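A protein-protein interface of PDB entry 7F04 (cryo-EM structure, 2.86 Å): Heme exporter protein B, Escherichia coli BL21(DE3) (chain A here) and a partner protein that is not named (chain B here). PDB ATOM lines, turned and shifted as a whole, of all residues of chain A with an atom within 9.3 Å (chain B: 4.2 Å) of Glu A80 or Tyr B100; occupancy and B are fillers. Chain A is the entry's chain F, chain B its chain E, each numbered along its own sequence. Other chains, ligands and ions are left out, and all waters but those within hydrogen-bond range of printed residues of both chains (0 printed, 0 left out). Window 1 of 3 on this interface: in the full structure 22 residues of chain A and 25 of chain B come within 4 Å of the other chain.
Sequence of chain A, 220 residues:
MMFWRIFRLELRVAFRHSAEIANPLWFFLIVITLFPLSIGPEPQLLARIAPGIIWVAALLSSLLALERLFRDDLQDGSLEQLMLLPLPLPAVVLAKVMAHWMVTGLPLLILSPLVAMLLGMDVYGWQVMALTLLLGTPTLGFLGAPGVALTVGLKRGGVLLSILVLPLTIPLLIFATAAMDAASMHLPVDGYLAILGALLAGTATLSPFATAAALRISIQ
The backbone carbonyl oxygen (O) of Gly B86 sits at hydrogen-bond distance from the side-chain hydroxyl (OH) of Tyr B100 (2.4 Å). O of Trp B80 sits at hydrogen-bond distance from NH1 of Arg B141 (3.3 Å). NH1 of Arg B102 lies within hydrogen-bond range of NE2 of His B101.
Glu A80 touches just these residues of chain B: Trp B80, Tyr B100 and Arg B141. Of the printed residues of chain A, Tyr B100 touches Glu A80. Of chain A, only Asp A76 and Gly A77 come within 4 Å of Gly B86. Printed residues of chain B within 4 Å of Asp A76: Gly B86. Printed residues of chain B within 4 Å of Arg A5: His B98 (3.8 Å), Phe B99 (3.5 Å), His B101 (2.5 Å) and Arg B102 (3.5 Å). Printed residues of chain B within 4 Å of Leu A9: Phe B99 (3.9 Å). Printed residues of chain A within 4 Å of Arg B102: Arg A5. Of the printed residues of chain A, Trp B80 touches Leu A79, Glu A80 and Met A83. The nearest printed residue of chain B that does not touch Glu A80 is Gly B86 (4.3 Å).
O of Trp B80 lies close to OE2 of Glu A80 (2.7 Å). O of His B101 sits at hydrogen-bond distance from NH1 of Arg A5. The backbone carbonyl oxygen (O) of Arg B102 lies within hydrogen-bond range of the guanidinium group (NH2) of Arg A5, 3.5 Å away. The guanidinium group of Arg B141 is in salt-bridge range of the side-chain carboxylate of Glu A80. N of Gly B86 lies close to O of Asp A76 (3.3 Å).
Met A1 touches Phe B99 (N to CE1, 3.9 Å). NH1 of Arg A5 touches O of His B98, at 3.8 Å. O of Phe B99 touches CD of Arg A5 (3.5 Å). Ile A6 touches Phe B99 (CG1 to CZ, 3.7 Å). CD1 of Leu A9 touches CB of Phe B99, 3.9 Å away. Gly B86 touches Gly A77 (CA to CA, 3.9 Å). Leu A79 touches Trp B80. CG of Glu A80 touches OH of Tyr B100, at 3.96 Å. Met A83 touches Trp B80 (CE to CB, 3.3 Å). Leu A84 touches Arg B141.
Of the 23 printed residues of chain A, 10 touch a printed residue of chain B. Hydrophobic or aromatic side chains of chain A that line the printed part of chain B: Ile A6, Leu A9, Leu A79, Met A83 and Leu A84. Among the printed residues, 15 pairs touch across the chains.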
ATOM      1  N   MET A   1      -2.926   2.888  14.410  1.00  0.00           N
ATOM      2  CA  MET A   1      -3.452   3.839  15.379  1.00  0.00           C
ATOM      3  C   MET A   1      -3.711   3.129  16.702  1.00  0.00           C
ATOM      4  O   MET A   1      -3.622   3.732  17.770  1.00  0.00           O
ATOM      5  CB  MET A   1      -4.725   4.503  14.839  1.00  0.00           C
ATOM      6  CG  MET A   1      -5.346   5.580  15.733  1.00  0.00           C
ATOM      7  SD  MET A   1      -6.395   4.982  17.075  1.00  0.00           S
ATOM      8  CE  MET A   1      -7.833   4.439  16.156  1.00  0.00           C
ATOM      9  N   MET A   2      -4.018   1.839  16.621  1.00  0.00           N
ATOM     10  CA  MET A   2      -4.232   1.032  17.808  1.00  0.00           C
ATOM     11  C   MET A   2      -2.899   0.679  18.459  1.00  0.00           C
ATOM     12  O   MET A   2      -1.828   0.828  17.869  1.00  0.00           O
ATOM     13  CB  MET A   2      -4.994  -0.247  17.464  1.00  0.00           C
ATOM     14  CG  MET A   2      -6.410  -0.023  16.964  1.00  0.00           C
ATOM     15  SD  MET A   2      -7.499   0.729  18.185  1.00  0.00           S
ATOM     16  CE  MET A   2      -8.951   1.046  17.189  1.00  0.00           C
ATOM     17  N   ARG A   5      -1.966  -2.635  16.792  1.00  0.00           N
ATOM     18  CA  ARG A   5      -1.592  -2.346  15.413  1.00  0.00           C
ATOM     19  C   ARG A   5      -0.159  -1.838  15.330  1.00  0.00           C
ATOM     20  O   ARG A   5       0.607  -2.264  14.460  1.00  0.00           O
ATOM     21  CB  ARG A   5      -2.563  -1.332  14.814  1.00  0.00           C
ATOM     22  CG  ARG A   5      -2.596  -1.318  13.303  1.00  0.00           C
ATOM     23  CD  ARG A   5      -3.195  -0.027  12.794  1.00  0.00           C
ATOM     24  NE  ARG A   5      -4.536   0.183  13.323  1.00  0.00           N
ATOM     25  CZ  ARG A   5      -5.633   0.229  12.582  1.00  0.00           C
ATOM     26  NH1 ARG A   5      -5.582   0.099  11.267  1.00  0.00           N
ATOM     27  NH2 ARG A   5      -6.808   0.412  13.175  1.00  0.00           N
ATOM     28  N   ILE A   6       0.225  -0.935  16.235  1.00  0.00           N
ATOM     29  CA  ILE A   6       1.601  -0.450  16.274  1.00  0.00           C
ATOM     30  C   ILE A   6       2.555  -1.578  16.647  1.00  0.00           C
ATOM     31  O   ILE A   6       3.655  -1.690  16.093  1.00  0.00           O
ATOM     32  CB  ILE A   6       1.724   0.738  17.246  1.00  0.00           C
ATOM     33  CG1 ILE A   6       0.936   1.939  16.728  1.00  0.00           C
ATOM     34  CG2 ILE A   6       3.177   1.120  17.451  1.00  0.00           C
ATOM     35  CD1 ILE A   6       0.754   3.026  17.755  1.00  0.00           C
ATOM     36  N   LEU A   9       2.955  -3.707  13.569  1.00  0.00           N
ATOM     37  CA  LEU A   9       3.726  -2.992  12.559  1.00  0.00           C
ATOM     38  C   LEU A   9       5.211  -3.014  12.884  1.00  0.00           C
ATOM     39  O   LEU A   9       6.044  -3.223  11.996  1.00  0.00           O
ATOM     40  CB  LEU A   9       3.233  -1.553  12.435  1.00  0.00           C
ATOM     41  CG  LEU A   9       3.889  -0.748  11.312  1.00  0.00           C
ATOM     42  CD1 LEU A   9       3.101  -0.889  10.021  1.00  0.00           C
ATOM     43  CD2 LEU A   9       4.037   0.710  11.705  1.00  0.00           C
ATOM     44  N   ASP A  73      12.905   5.831  12.215  1.00  0.00           N
ATOM     45  CA  ASP A  73      11.648   6.542  12.392  1.00  0.00           C
ATOM     46  C   ASP A  73      11.817   8.043  12.253  1.00  0.00           C
ATOM     47  O   ASP A  73      10.935   8.708  11.711  1.00  0.00           O
ATOM     48  CB  ASP A  73      11.039   6.215  13.765  1.00  0.00           C
ATOM     49  CG  ASP A  73      10.125   5.010  13.726  1.00  0.00           C
ATOM     50  OD1 ASP A  73       9.355   4.878  12.754  1.00  0.00           O
ATOM     51  OD2 ASP A  73      10.176   4.193  14.667  1.00  0.00           O
ATOM     52  N   ASP A  76      11.908   9.118   8.522  1.00  0.00           N
ATOM     53  CA  ASP A  76      10.634   9.068   7.816  1.00  0.00           C
ATOM     54  C   ASP A  76       9.432   9.345   8.712  1.00  0.00           C
ATOM     55  O   ASP A  76       8.695  10.300   8.456  1.00  0.00           O
ATOM     56  CB  ASP A  76      10.506   7.712   7.104  1.00  0.00           C
ATOM     57  CG  ASP A  76      10.495   6.533   8.065  1.00  0.00           C
ATOM     58  OD1 ASP A  76      10.625   6.747   9.286  1.00  0.00           O
ATOM     59  OD2 ASP A  76      10.369   5.383   7.598  1.00  0.00           O
ATOM     60  N   GLY A  77       9.219   8.562   9.769  1.00  0.00           N
ATOM     61  CA  GLY A  77       7.936   8.576  10.445  1.00  0.00           C
ATOM     62  C   GLY A  77       7.936   8.408  11.952  1.00  0.00           C
ATOM     63  O   GLY A  77       7.092   7.681  12.481  1.00  0.00           O
ATOM     64  N   SER A  78       8.883   9.035  12.655  1.00  0.00           N
ATOM     65  CA  SER A  78       8.763   9.122  14.108  1.00  0.00           C
ATOM     66  C   SER A  78       7.530   9.925  14.489  1.00  0.00           C
ATOM     67  O   SER A  78       6.778   9.538  15.389  1.00  0.00           O
ATOM     68  CB  SER A  78      10.020   9.743  14.716  1.00  0.00           C
ATOM     69  OG  SER A  78      10.062   9.534  16.117  1.00  0.00           O
ATOM     70  N   LEU A  79       7.301  11.040  13.801  1.00  0.00           N
ATOM     71  CA  LEU A  79       5.998  11.680  13.802  1.00  0.00           C
ATOM     72  C   LEU A  79       5.003  10.780  13.068  1.00  0.00           C
ATOM     73  O   LEU A  79       5.322   9.660  12.665  1.00  0.00           O
ATOM     74  CB  LEU A  79       6.107  13.083  13.206  1.00  0.00           C
ATOM     75  CG  LEU A  79       6.576  13.306  11.761  1.00  0.00           C
ATOM     76  CD1 LEU A  79       5.464  13.148  10.739  1.00  0.00           C
ATOM     77  CD2 LEU A  79       7.236  14.673  11.627  1.00  0.00           C
ATOM     78  N   GLU A  80       3.772  11.263  12.914  1.00  0.00           N
ATOM     79  CA  GLU A  80       2.588  10.479  12.562  1.00  0.00           C
ATOM     80  C   GLU A  80       2.153   9.599  13.719  1.00  0.00           C
ATOM     81  O   GLU A  80       1.093   8.974  13.643  1.00  0.00           O
ATOM     82  CB  GLU A  80       2.767   9.596  11.315  1.00  0.00           C
ATOM     83  CG  GLU A  80       3.436  10.261  10.131  1.00  0.00           C
ATOM     84  CD  GLU A  80       2.517  11.205   9.399  1.00  0.00           C
ATOM     85  OE1 GLU A  80       1.286  11.070   9.541  1.00  0.00           O
ATOM     86  OE2 GLU A  80       3.032  12.080   8.675  1.00  0.00           O
ATOM     87  N   GLN A  81       2.941   9.530  14.789  1.00  0.00           N
ATOM     88  CA  GLN A  81       2.581   8.863  16.031  1.00  0.00           C
ATOM     89  C   GLN A  81       2.506   9.847  17.184  1.00  0.00           C
ATOM     90  O   GLN A  81       1.608   9.746  18.028  1.00  0.00           O
ATOM     91  CB  GLN A  81       3.592   7.751  16.341  1.00  0.00           C
ATOM     92  CG  GLN A  81       3.665   6.684  15.267  1.00  0.00           C
ATOM     93  CD  GLN A  81       4.752   5.669  15.526  1.00  0.00           C
ATOM     94  OE1 GLN A  81       5.548   5.817  16.450  1.00  0.00           O
ATOM     95  NE2 GLN A  81       4.791   4.627  14.709  1.00  0.00           N
ATOM     96  N   LEU A  82       3.441  10.796  17.250  1.00  0.00           N
ATOM     97  CA  LEU A  82       3.275  11.937  18.140  1.00  0.00           C
ATOM     98  C   LEU A  82       2.130  12.823  17.670  1.00  0.00           C
ATOM     99  O   LEU A  82       1.242  13.178  18.452  1.00  0.00           O
ATOM    100  CB  LEU A  82       4.571  12.749  18.198  1.00  0.00           C
ATOM    101  CG  LEU A  82       5.803  12.227  18.938  1.00  0.00           C
ATOM    102  CD1 LEU A  82       6.610  11.294  18.062  1.00  0.00           C
ATOM    103  CD2 LEU A  82       6.662  13.391  19.383  1.00  0.00           C
ATOM    104  N   MET A  83       2.137  13.175  16.386  1.00  0.00           N
ATOM    105  CA  MET A  83       1.193  14.118  15.802  1.00  0.00           C
ATOM    106  C   MET A  83      -0.183  13.513  15.564  1.00  0.00           C
ATOM    107  O   MET A  83      -1.169  14.252  15.489  1.00  0.00           O
ATOM    108  CB  MET A  83       1.778  14.641  14.489  1.00  0.00           C
ATOM    109  CG  MET A  83       0.931  15.604  13.697  1.00  0.00           C
ATOM    110  SD  MET A  83      -0.157  14.681  12.605  1.00  0.00           S
ATOM    111  CE  MET A  83       1.013  13.511  11.930  1.00  0.00           C
ATOM    112  N   LEU A  84      -0.274  12.194  15.465  1.00  0.00           N
ATOM    113  CA  LEU A  84      -1.524  11.534  15.120  1.00  0.00           C
ATOM    114  C   LEU A  84      -1.747  10.393  16.093  1.00  0.00           C
ATOM    115  O   LEU A  84      -1.107  10.352  17.148  1.00  0.00           O
ATOM    116  CB  LEU A  84      -1.491  11.022  13.679  1.00  0.00           C
ATOM    117  CG  LEU A  84      -2.182  11.853  12.596  1.00  0.00           C
ATOM    118  CD1 LEU A  84      -1.893  11.272  11.226  1.00  0.00           C
ATOM    119  CD2 LEU A  84      -3.674  11.917  12.837  1.00  0.00           C
ATOM    120  N   LEU A  85      -2.652   9.475  15.757  1.00  0.00           N
ATOM    121  CA  LEU A  85      -2.849   8.285  16.571  1.00  0.00           C
ATOM    122  C   LEU A  85      -3.268   8.691  17.976  1.00  0.00           C
ATOM    123  O   LEU A  85      -2.429   8.717  18.882  1.00  0.00           O
ATOM    124  CB  LEU A  85      -1.587   7.419  16.616  1.00  0.00           C
ATOM    125  CG  LEU A  85      -0.852   7.120  15.310  1.00  0.00           C
ATOM    126  CD1 LEU A  85       0.111   5.967  15.513  1.00  0.00           C
ATOM    127  CD2 LEU A  85      -1.814   6.819  14.175  1.00  0.00           C
ATOM    128  N   PRO A  86      -4.539   9.052  18.187  1.00  0.00           N
ATOM    129  CA  PRO A  86      -4.977   9.563  19.495  1.00  0.00           C
ATOM    130  C   PRO A  86      -4.561   8.708  20.687  1.00  0.00           C
ATOM    131  O   PRO A  86      -4.735   9.117  21.839  1.00  0.00           O
ATOM    132  CB  PRO A  86      -6.504   9.597  19.356  1.00  0.00           C
ATOM    133  CG  PRO A  86      -6.747   9.708  17.901  1.00  0.00           C
ATOM    134  CD  PRO A  86      -5.653   8.945  17.232  1.00  0.00           C
ATOM    135  N   LEU A  87      -4.032   7.521  20.421  1.00  0.00           N
ATOM    136  CA  LEU A  87      -3.358   6.747  21.449  1.00  0.00           C
ATOM    137  C   LEU A  87      -2.210   7.563  22.037  1.00  0.00           C
ATOM    138  O   LEU A  87      -1.399   8.114  21.282  1.00  0.00           O
ATOM    139  CB  LEU A  87      -2.831   5.444  20.850  1.00  0.00           C
ATOM    140  CG  LEU A  87      -2.147   4.428  21.759  1.00  0.00           C
ATOM    141  CD1 LEU A  87      -3.172   3.550  22.449  1.00  0.00           C
ATOM    142  CD2 LEU A  87      -1.172   3.587  20.959  1.00  0.00           C
ATOM    143  N   LEU A  89       1.280   8.939  23.512  1.00  0.00           N
ATOM    144  CA  LEU A  89       2.659   8.598  23.169  1.00  0.00           C
ATOM    145  C   LEU A  89       3.304   7.592  24.117  1.00  0.00           C
ATOM    146  O   LEU A  89       4.085   6.754  23.631  1.00  0.00           O
ATOM    147  CB  LEU A  89       3.503   9.875  23.078  1.00  0.00           C
ATOM    148  CG  LEU A  89       4.878   9.716  22.427  1.00  0.00           C
ATOM    149  CD1 LEU A  89       4.744   9.178  21.015  1.00  0.00           C
ATOM    150  CD2 LEU A  89       5.632  11.032  22.426  1.00  0.00           C
ATOM    151  N   VAL A  92       2.341   4.327  22.732  1.00  0.00           N
ATOM    152  CA  VAL A  92       3.092   4.031  21.514  1.00  0.00           C
ATOM    153  C   VAL A  92       4.481   3.519  21.863  1.00  0.00           C
ATOM    154  O   VAL A  92       4.971   2.545  21.275  1.00  0.00           O
ATOM    155  CB  VAL A  92       3.160   5.278  20.616  1.00  0.00           C
ATOM    156  CG1 VAL A  92       4.009   5.008  19.389  1.00  0.00           C
ATOM    157  CG2 VAL A  92       1.765   5.727  20.221  1.00  0.00           C
ATOM    158  N   LYS A  96       6.069  -0.180  21.015  1.00  0.00           N
ATOM    159  CA  LYS A  96       7.327  -0.319  20.291  1.00  0.00           C
ATOM    160  C   LYS A  96       8.359  -1.090  21.104  1.00  0.00           C
ATOM    161  O   LYS A  96       9.112  -1.897  20.551  1.00  0.00           O
ATOM    162  CB  LYS A  96       7.859   1.058  19.901  1.00  0.00           C
ATOM    163  CG  LYS A  96       7.022   1.748  18.840  1.00  0.00           C
ATOM    164  CD  LYS A  96       7.646   3.059  18.420  1.00  0.00           C
ATOM    165  CE  LYS A  96       8.681   2.847  17.335  1.00  0.00           C
ATOM    166  NZ  LYS A  96       8.076   2.934  15.985  1.00  0.00           N
ATOM    167  N   ARG A 216       9.629  13.747  22.464  1.00  0.00           N
ATOM    168  CA  ARG A 216       9.134  15.099  22.228  1.00  0.00           C
ATOM    169  C   ARG A 216      10.280  16.100  22.176  1.00  0.00           C
ATOM    170  O   ARG A 216      10.260  17.037  21.370  1.00  0.00           O
ATOM    171  CB  ARG A 216       8.127  15.490  23.307  1.00  0.00           C
ATOM    172  CG  ARG A 216       6.858  14.663  23.287  1.00  0.00           C
ATOM    173  CD  ARG A 216       5.631  15.508  23.564  1.00  0.00           C
ATOM    174  NE  ARG A 216       4.417  14.873  23.065  1.00  0.00           N
ATOM    175  CZ  ARG A 216       3.960  14.999  21.827  1.00  0.00           C
ATOM    176  NH1 ARG A 216       4.581  15.751  20.934  1.00  0.00           N
ATOM    177  NH2 ARG A 216       2.852  14.354  21.477  1.00  0.00           N
ATOM    178  N   ILE A 219      12.134  15.463  18.678  1.00  0.00           N
ATOM    179  CA  ILE A 219      11.417  15.761  17.442  1.00  0.00           C
ATOM    180  C   ILE A 219      11.531  17.239  17.087  1.00  0.00           C
ATOM    181  O   ILE A 219      11.436  17.609  15.910  1.00  0.00           O
ATOM    182  CB  ILE A 219       9.946  15.311  17.552  1.00  0.00           C
ATOM    183  CG1 ILE A 219       9.335  15.138  16.162  1.00  0.00           C
ATOM    184  CG2 ILE A 219       9.129  16.306  18.358  1.00  0.00           C
ATOM    185  CD1 ILE A 219       9.925  13.989  15.379  1.00  0.00           C
ATOM    186  N   TRP B  80      -1.311  15.062   8.520  1.00  0.00           N
ATOM    187  CA  TRP B  80       0.022  15.578   8.226  1.00  0.00           C
ATOM    188  C   TRP B  80       0.775  14.660   7.283  1.00  0.00           C
ATOM    189  O   TRP B  80       0.936  13.467   7.560  1.00  0.00           O
ATOM    190  CB  TRP B  80       0.812  15.785   9.518  1.00  0.00           C
ATOM    191  CG  TRP B  80       2.200  16.329   9.375  1.00  0.00           C
ATOM    192  CD1 TRP B  80       3.352  15.606   9.480  1.00  0.00           C
ATOM    193  CD2 TRP B  80       2.596  17.650   9.006  1.00  0.00           C
ATOM    194  NE1 TRP B  80       4.440  16.402   9.260  1.00  0.00           N
ATOM    195  CE2 TRP B  80       4.006  17.664   8.958  1.00  0.00           C
ATOM    196  CE3 TRP B  80       1.904  18.827   8.729  1.00  0.00           C
ATOM    197  CZ2 TRP B  80       4.730  18.804   8.647  1.00  0.00           C
ATOM    198  CZ3 TRP B  80       2.629  19.954   8.419  1.00  0.00           C
ATOM    199  CH2 TRP B  80       4.027  19.939   8.384  1.00  0.00           C
ATOM    200  N   GLY B  86       6.680   9.721   5.850  1.00  0.00           N
ATOM    201  CA  GLY B  86       6.114   9.042   6.995  1.00  0.00           C
ATOM    202  C   GLY B  86       5.743   7.602   6.752  1.00  0.00           C
ATOM    203  O   GLY B  86       4.819   7.093   7.396  1.00  0.00           O
ATOM    204  N   ASN B  96       1.962  -0.186   4.125  1.00  0.00           N
ATOM    205  CA  ASN B  96       2.107   1.130   4.739  1.00  0.00           C
ATOM    206  C   ASN B  96       0.765   1.842   4.840  1.00  0.00           C
ATOM    207  O   ASN B  96       0.465   2.469   5.861  1.00  0.00           O
ATOM    208  CB  ASN B  96       3.107   1.968   3.946  1.00  0.00           C
ATOM    209  CG  ASN B  96       4.490   1.944   4.553  1.00  0.00           C
ATOM    210  OD1 ASN B  96       4.646   2.053   5.767  1.00  0.00           O
ATOM    211  ND2 ASN B  96       5.502   1.796   3.714  1.00  0.00           N
ATOM    212  N   LEU B  97      -0.055   1.759   3.791  1.00  0.00           N
ATOM    213  CA  LEU B  97      -1.370   2.388   3.823  1.00  0.00           C
ATOM    214  C   LEU B  97      -2.343   1.590   4.679  1.00  0.00           C
ATOM    215  O   LEU B  97      -3.327   2.143   5.183  1.00  0.00           O
ATOM    216  CB  LEU B  97      -1.900   2.541   2.398  1.00  0.00           C
ATOM    217  CG  LEU B  97      -3.173   3.361   2.221  1.00  0.00           C
ATOM    218  CD1 LEU B  97      -2.922   4.789   2.652  1.00  0.00           C
ATOM    219  CD2 LEU B  97      -3.646   3.313   0.784  1.00  0.00           C
ATOM    220  N   HIS B  98      -2.085   0.293   4.844  1.00  0.00           N
ATOM    221  CA  HIS B  98      -2.892  -0.537   5.728  1.00  0.00           C
ATOM    222  C   HIS B  98      -2.809  -0.057   7.170  1.00  0.00           C
ATOM    223  O   HIS B  98      -3.756  -0.241   7.942  1.00  0.00           O
ATOM    224  CB  HIS B  98      -2.411  -1.985   5.611  1.00  0.00           C
ATOM    225  CG  HIS B  98      -3.180  -2.966   6.438  1.00  0.00           C
ATOM    226  ND1 HIS B  98      -4.450  -3.387   6.112  1.00  0.00           N
ATOM    227  CD2 HIS B  98      -2.847  -3.621   7.574  1.00  0.00           C
ATOM    228  CE1 HIS B  98      -4.865  -4.262   7.010  1.00  0.00           C
ATOM    229  NE2 HIS B  98      -3.910  -4.421   7.909  1.00  0.00           N
ATOM    230  N   PHE B  99      -1.687   0.561   7.547  1.00  0.00           N
ATOM    231  CA  PHE B  99      -1.493   1.009   8.922  1.00  0.00           C
ATOM    232  C   PHE B  99      -2.327   2.241   9.244  1.00  0.00           C
ATOM    233  O   PHE B  99      -2.668   2.468  10.410  1.00  0.00           O
ATOM    234  CB  PHE B  99      -0.011   1.297   9.166  1.00  0.00           C
ATOM    235  CG  PHE B  99       0.291   1.806  10.547  1.00  0.00           C
ATOM    236  CD1 PHE B  99       0.065   1.012  11.656  1.00  0.00           C
ATOM    237  CD2 PHE B  99       0.807   3.075  10.734  1.00  0.00           C
ATOM    238  CE1 PHE B  99       0.343   1.474  12.924  1.00  0.00           C
ATOM    239  CE2 PHE B  99       1.087   3.543  12.001  1.00  0.00           C
ATOM    240  CZ  PHE B  99       0.854   2.741  13.097  1.00  0.00           C
ATOM    241  N   TYR B 100      -2.661   3.045   8.240  1.00  0.00           N
ATOM    242  CA  TYR B 100      -3.331   4.320   8.452  1.00  0.00           C
ATOM    243  C   TYR B 100      -4.845   4.251   8.298  1.00  0.00           C
ATOM    244  O   TYR B 100      -5.505   5.286   8.416  1.00  0.00           O
ATOM    245  CB  TYR B 100      -2.778   5.369   7.486  1.00  0.00           C
ATOM    246  CG  TYR B 100      -1.341   5.749   7.737  1.00  0.00           C
ATOM    247  CD1 TYR B 100      -0.987   6.532   8.825  1.00  0.00           C
ATOM    248  CD2 TYR B 100      -0.336   5.326   6.884  1.00  0.00           C
ATOM    249  CE1 TYR B 100       0.327   6.883   9.055  1.00  0.00           C
ATOM    250  CE2 TYR B 100       0.978   5.671   7.105  1.00  0.00           C
ATOM    251  CZ  TYR B 100       1.305   6.449   8.190  1.00  0.00           C
ATOM    252  OH  TYR B 100       2.617   6.792   8.409  1.00  0.00           O
ATOM    253  N   HIS B 101      -5.415   3.082   8.039  1.00  0.00           N
ATOM    254  CA  HIS B 101      -6.853   2.961   7.856  1.00  0.00           C
ATOM    255  C   HIS B 101      -7.500   2.369   9.099  1.00  0.00           C
ATOM    256  O   HIS B 101      -6.995   1.404   9.679  1.00  0.00           O
ATOM    257  CB  HIS B 101      -7.189   2.104   6.638  1.00  0.00           C
ATOM    258  CG  HIS B 101      -8.536   2.396   6.058  1.00  0.00           C
ATOM    259  ND1 HIS B 101      -9.158   1.563   5.156  1.00  0.00           N
ATOM    260  CD2 HIS B 101      -9.385   3.432   6.259  1.00  0.00           C
ATOM    261  CE1 HIS B 101     -10.330   2.071   4.823  1.00  0.00           C
ATOM    262  NE2 HIS B 101     -10.492   3.206   5.478  1.00  0.00           N
ATOM    263  N   ARG B 102      -8.628   2.958   9.501  1.00  0.00           N
ATOM    264  CA  ARG B 102      -9.282   2.549  10.737  1.00  0.00           C
ATOM    265  C   ARG B 102      -9.963   1.187  10.599  1.00  0.00           C
ATOM    266  O   ARG B 102      -9.826   0.336  11.485  1.00  0.00           O
ATOM    267  CB  ARG B 102     -10.274   3.628  11.185  1.00  0.00           C
ATOM    268  CG  ARG B 102     -11.555   3.737  10.364  1.00  0.00           C
ATOM    269  CD  ARG B 102     -11.357   4.538   9.088  1.00  0.00           C
ATOM    270  NE  ARG B 102     -12.612   4.739   8.373  1.00  0.00           N
ATOM    271  CZ  ARG B 102     -12.706   5.259   7.157  1.00  0.00           C
ATOM    272  NH1 ARG B 102     -11.642   5.704   6.511  1.00  0.00           N
ATOM    273  NH2 ARG B 102     -13.901   5.340   6.578  1.00  0.00           N
ATOM    274  N   ARG B 141      -3.332   8.516   1.359  1.00  0.00           N
ATOM    275  CA  ARG B 141      -4.180   8.725   2.524  1.00  0.00           C
ATOM    276  C   ARG B 141      -5.223   9.803   2.289  1.00  0.00           C
ATOM    277  O   ARG B 141      -6.222   9.849   3.012  1.00  0.00           O
ATOM    278  CB  ARG B 141      -3.327   9.092   3.735  1.00  0.00           C
ATOM    279  CG  ARG B 141      -2.278   8.064   4.083  1.00  0.00           C
ATOM    280  CD  ARG B 141      -1.160   8.682   4.887  1.00  0.00           C
ATOM    281  NE  ARG B 141      -1.640   9.218   6.153  1.00  0.00           N
ATOM    282  CZ  ARG B 141      -0.943  10.033   6.928  1.00  0.00           C
ATOM    283  NH1 ARG B 141       0.274  10.430   6.595  1.00  0.00           N
ATOM    284  NH2 ARG B 141      -1.477  10.460   8.067  1.00  0.00           N
